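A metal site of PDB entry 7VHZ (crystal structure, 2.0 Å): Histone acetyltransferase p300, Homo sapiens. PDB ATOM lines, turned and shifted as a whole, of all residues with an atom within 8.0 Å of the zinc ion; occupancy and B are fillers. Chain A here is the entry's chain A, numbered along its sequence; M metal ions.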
ATOM      1  N   LEU A  19     -35.994 -21.936  13.506  1.00  0.00           N
ATOM      2  CA  LEU A  19     -35.984 -21.641  12.083  1.00  0.00           C
ATOM      3  C   LEU A  19     -35.408 -22.802  11.282  1.00  0.00           C
ATOM      4  O   LEU A  19     -34.581 -23.563  11.784  1.00  0.00           O
ATOM      5  CB  LEU A  19     -35.186 -20.355  11.777  1.00  0.00           C
ATOM      6  CG  LEU A  19     -35.416 -19.140  12.669  1.00  0.00           C
ATOM      7  CD1 LEU A  19     -34.236 -18.189  12.573  1.00  0.00           C
ATOM      8  CD2 LEU A  19     -36.710 -18.430  12.270  1.00  0.00           C
ATOM      9  N   CYS A  20     -35.830 -22.912  10.026  1.00  0.00           N
ATOM     10  CA  CYS A  20     -35.239 -23.833   9.062  1.00  0.00           C
ATOM     11  C   CYS A  20     -33.895 -23.292   8.575  1.00  0.00           C
ATOM     12  O   CYS A  20     -33.656 -22.069   8.592  1.00  0.00           O
ATOM     13  CB  CYS A  20     -36.173 -24.075   7.880  1.00  0.00           C
ATOM     14  SG  CYS A  20     -37.186 -22.655   7.418  1.00  0.00           S
ATOM     15  N   CYS A  21     -33.008 -24.195   8.152  1.00  0.00           N
ATOM     16  CA  CYS A  21     -31.672 -23.793   7.707  1.00  0.00           C
ATOM     17  C   CYS A  21     -31.445 -23.836   6.201  1.00  0.00           C
ATOM     18  O   CYS A  21     -30.375 -23.435   5.744  1.00  0.00           O
ATOM     19  CB  CYS A  21     -30.625 -24.647   8.431  1.00  0.00           C
ATOM     20  SG  CYS A  21     -29.660 -25.724   7.394  1.00  0.00           S
ATOM     21  N   TYR A  22     -32.411 -24.334   5.416  1.00  0.00           N
ATOM     22  CA  TYR A  22     -32.418 -24.210   3.960  1.00  0.00           C
ATOM     23  C   TYR A  22     -31.289 -24.946   3.229  1.00  0.00           C
ATOM     24  O   TYR A  22     -31.345 -25.093   2.000  1.00  0.00           O
ATOM     25  CB  TYR A  22     -32.374 -22.730   3.549  1.00  0.00           C
ATOM     26  CG  TYR A  22     -32.711 -22.469   2.096  1.00  0.00           C
ATOM     27  CD1 TYR A  22     -34.029 -22.387   1.669  1.00  0.00           C
ATOM     28  CD2 TYR A  22     -31.699 -22.306   1.138  1.00  0.00           C
ATOM     29  CE1 TYR A  22     -34.348 -22.166   0.343  1.00  0.00           C
ATOM     30  CE2 TYR A  22     -32.006 -22.085  -0.202  1.00  0.00           C
ATOM     31  CZ  TYR A  22     -33.330 -22.014  -0.595  1.00  0.00           C
ATOM     32  OH  TYR A  22     -33.646 -21.792  -1.912  1.00  0.00           O
ATOM     33  N   GLY A  23     -30.305 -25.457   3.950  1.00  0.00           N
ATOM     34  CA  GLY A  23     -29.248 -26.188   3.256  1.00  0.00           C
ATOM     35  C   GLY A  23     -29.183 -27.623   3.709  1.00  0.00           C
ATOM     36  O   GLY A  23     -28.154 -28.288   3.592  1.00  0.00           O
ATOM     37  N   LYS A  24     -30.309 -28.111   4.211  1.00  0.00           N
ATOM     38  CA  LYS A  24     -30.500 -29.508   4.551  1.00  0.00           C
ATOM     39  C   LYS A  24     -31.978 -29.750   4.849  1.00  0.00           C
ATOM     40  O   LYS A  24     -32.562 -29.033   5.655  1.00  0.00           O
ATOM     41  CB  LYS A  24     -29.651 -29.910   5.752  1.00  0.00           C
ATOM     42  CG  LYS A  24     -29.012 -31.271   5.669  1.00  0.00           C
ATOM     43  CD  LYS A  24     -27.586 -31.237   6.189  1.00  0.00           C
ATOM     44  CE  LYS A  24     -27.539 -31.321   7.703  1.00  0.00           C
ATOM     45  NZ  LYS A  24     -26.149 -31.160   8.234  1.00  0.00           N
ATOM     46  N   GLN A  25     -32.605 -30.715   4.169  1.00  0.00           N
ATOM     47  CA  GLN A  25     -33.943 -31.100   4.580  1.00  0.00           C
ATOM     48  C   GLN A  25     -33.868 -31.650   6.000  1.00  0.00           C
ATOM     49  O   GLN A  25     -32.934 -32.361   6.357  1.00  0.00           O
ATOM     50  CB  GLN A  25     -34.536 -32.144   3.624  1.00  0.00           C
ATOM     51  N   LEU A  26     -34.866 -31.283   6.826  1.00  0.00           N
ATOM     52  CA  LEU A  26     -34.946 -31.674   8.227  1.00  0.00           C
ATOM     53  C   LEU A  26     -33.846 -31.074   9.091  1.00  0.00           C
ATOM     54  O   LEU A  26     -33.522 -31.613  10.152  1.00  0.00           O
ATOM     55  CB  LEU A  26     -34.957 -33.209   8.390  1.00  0.00           C
ATOM     56  N   CYS A  27     -33.205 -29.986   8.643  1.00  0.00           N
ATOM     57  CA  CYS A  27     -32.306 -29.202   9.484  1.00  0.00           C
ATOM     58  C   CYS A  27     -33.010 -27.954   9.992  1.00  0.00           C
ATOM     59  O   CYS A  27     -33.741 -27.283   9.253  1.00  0.00           O
ATOM     60  CB  CYS A  27     -31.038 -28.809   8.725  1.00  0.00           C
ATOM     61  SG  CYS A  27     -29.641 -28.366   9.803  1.00  0.00           S
ATOM     62  N   THR A  28     -32.787 -27.633  11.272  1.00  0.00           N
ATOM     63  CA  THR A  28     -33.392 -26.468  11.893  1.00  0.00           C
ATOM     64  C   THR A  28     -32.351 -25.716  12.708  1.00  0.00           C
ATOM     65  O   THR A  28     -31.345 -26.273  13.140  1.00  0.00           O
ATOM     66  CB  THR A  28     -34.574 -26.841  12.807  1.00  0.00           C
ATOM     67  OG1 THR A  28     -34.212 -27.956  13.632  1.00  0.00           O
ATOM     68  CG2 THR A  28     -35.801 -27.206  11.978  1.00  0.00           C
ATOM     69  N   ILE A  29     -32.598 -24.417  12.886  1.00  0.00           N
ATOM     70  CA  ILE A  29     -31.780 -23.542  13.723  1.00  0.00           C
ATOM     71  C   ILE A  29     -32.552 -23.308  15.024  1.00  0.00           C
ATOM     72  O   ILE A  29     -33.616 -22.666  14.987  1.00  0.00           O
ATOM     73  CB  ILE A  29     -31.457 -22.209  13.031  1.00  0.00           C
ATOM     74  CG1 ILE A  29     -30.986 -22.455  11.593  1.00  0.00           C
ATOM     75  CG2 ILE A  29     -30.406 -21.443  13.831  1.00  0.00           C
ATOM     76  CD1 ILE A  29     -31.017 -21.209  10.736  1.00  0.00           C
ATOM     77  N   HIS A  43     -32.060 -18.593   5.798  1.00  0.00           N
ATOM     78  CA  HIS A  43     -31.292 -18.722   7.020  1.00  0.00           C
ATOM     79  C   HIS A  43     -30.477 -20.003   6.968  1.00  0.00           C
ATOM     80  O   HIS A  43     -30.948 -21.023   6.467  1.00  0.00           O
ATOM     81  CB  HIS A  43     -32.209 -18.728   8.244  1.00  0.00           C
ATOM     82  CG  HIS A  43     -33.318 -17.730   8.165  1.00  0.00           C
ATOM     83  ND1 HIS A  43     -33.198 -16.441   8.655  1.00  0.00           N
ATOM     84  CD2 HIS A  43     -34.562 -17.812   7.631  1.00  0.00           C
ATOM     85  CE1 HIS A  43     -34.322 -15.784   8.432  1.00  0.00           C
ATOM     86  NE2 HIS A  43     -35.167 -16.593   7.810  1.00  0.00           N
ATOM     87  N   PHE A  44     -29.239 -19.956   7.467  1.00  0.00           N
ATOM     88  CA  PHE A  44     -28.345 -21.106   7.482  1.00  0.00           C
ATOM     89  C   PHE A  44     -27.781 -21.293   8.873  1.00  0.00           C
ATOM     90  O   PHE A  44     -27.227 -20.356   9.450  1.00  0.00           O
ATOM     91  CB  PHE A  44     -27.198 -20.934   6.482  1.00  0.00           C
ATOM     92  CG  PHE A  44     -27.606 -21.114   5.047  1.00  0.00           C
ATOM     93  CD1 PHE A  44     -28.326 -20.131   4.395  1.00  0.00           C
ATOM     94  CD2 PHE A  44     -27.269 -22.259   4.349  1.00  0.00           C
ATOM     95  CE1 PHE A  44     -28.704 -20.289   3.064  1.00  0.00           C
ATOM     96  CE2 PHE A  44     -27.644 -22.430   3.030  1.00  0.00           C
ATOM     97  CZ  PHE A  44     -28.369 -21.438   2.388  1.00  0.00           C
ATOM     98  N   CYS A  45     -27.902 -22.509   9.408  1.00  0.00           N
ATOM     99  CA  CYS A  45     -27.166 -22.844  10.615  1.00  0.00           C
ATOM    100  C   CYS A  45     -25.671 -22.814  10.322  1.00  0.00           C
ATOM    101  O   CYS A  45     -25.239 -22.971   9.180  1.00  0.00           O
ATOM    102  CB  CYS A  45     -27.593 -24.230  11.130  1.00  0.00           C
ATOM    103  SG  CYS A  45     -26.829 -25.646  10.302  1.00  0.00           S
ATOM    104  N   GLU A  46     -24.879 -22.568  11.370  1.00  0.00           N
ATOM    105  CA  GLU A  46     -23.441 -22.355  11.168  1.00  0.00           C
ATOM    106  C   GLU A  46     -22.776 -23.549  10.485  1.00  0.00           C
ATOM    107  O   GLU A  46     -21.926 -23.372   9.614  1.00  0.00           O
ATOM    108  CB  GLU A  46     -22.773 -22.058  12.506  1.00  0.00           C
ATOM    109  CG  GLU A  46     -21.400 -21.415  12.359  1.00  0.00           C
ATOM    110  CD  GLU A  46     -20.879 -20.838  13.659  1.00  0.00           C
ATOM    111  OE1 GLU A  46     -21.413 -21.209  14.724  1.00  0.00           O
ATOM    112  OE2 GLU A  46     -19.946 -20.014  13.617  1.00  0.00           O
ATOM    113  N   LYS A  47     -23.166 -24.768  10.875  1.00  0.00           N
ATOM    114  CA  LYS A  47     -22.552 -25.956  10.286  1.00  0.00           C
ATOM    115  C   LYS A  47     -22.827 -26.050   8.798  1.00  0.00           C
ATOM    116  O   LYS A  47     -21.904 -26.229   7.993  1.00  0.00           O
ATOM    117  CB  LYS A  47     -23.033 -27.215  11.013  1.00  0.00           C
ATOM    118  N   CYS A  48     -24.102 -25.938   8.409  1.00  0.00           N
ATOM    119  CA  CYS A  48     -24.448 -26.032   6.989  1.00  0.00           C
ATOM    120  C   CYS A  48     -23.817 -24.926   6.168  1.00  0.00           C
ATOM    121  O   CYS A  48     -23.573 -25.096   4.966  1.00  0.00           O
ATOM    122  CB  CYS A  48     -25.974 -26.026   6.828  1.00  0.00           C
ATOM    123  SG  CYS A  48     -26.779 -27.618   7.159  1.00  0.00           S
ATOM    124  N   PHE A  49     -23.537 -23.775   6.797  1.00  0.00           N
ATOM    125  CA  PHE A  49     -22.972 -22.635   6.078  1.00  0.00           C
ATOM    126  C   PHE A  49     -21.485 -22.815   5.776  1.00  0.00           C
ATOM    127  O   PHE A  49     -21.046 -22.577   4.637  1.00  0.00           O
ATOM    128  CB  PHE A  49     -23.188 -21.363   6.896  1.00  0.00           C
ATOM    129  CG  PHE A  49     -23.096 -20.089   6.100  1.00  0.00           C
ATOM    130  CD1 PHE A  49     -24.117 -19.713   5.242  1.00  0.00           C
ATOM    131  CD2 PHE A  49     -21.988 -19.263   6.215  1.00  0.00           C
ATOM    132  CE1 PHE A  49     -24.040 -18.541   4.505  1.00  0.00           C
ATOM    133  CE2 PHE A  49     -21.895 -18.088   5.485  1.00  0.00           C
ATOM    134  CZ  PHE A  49     -22.928 -17.728   4.632  1.00  0.00           C
HETATM  135 ZN    ZN M   1     -28.205 -26.807   8.836  1.00  0.00          ZN
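Four residues have an atom within 4 Å of the zinc ion: Cys 21, Cys 27, Cys 45 and Cys 48.
The nearest printed residue that does not touch the zinc ion is Lys 24 (4.6 Å).
The zinc ion is bound by SG of Cys 21, SG of Cys 45, SG of Cys 27 and SG of Cys 48.
SG of Cys 21 sits close to N of Gly 23 (3.5 Å).
SG of Cys 48 lies close to NZ of Lys 24 (3.8 Å).
The backbone carbonyl oxygen (O) of Cys 21 lies close to the backbone carbonyl oxygen (O) of His 43.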
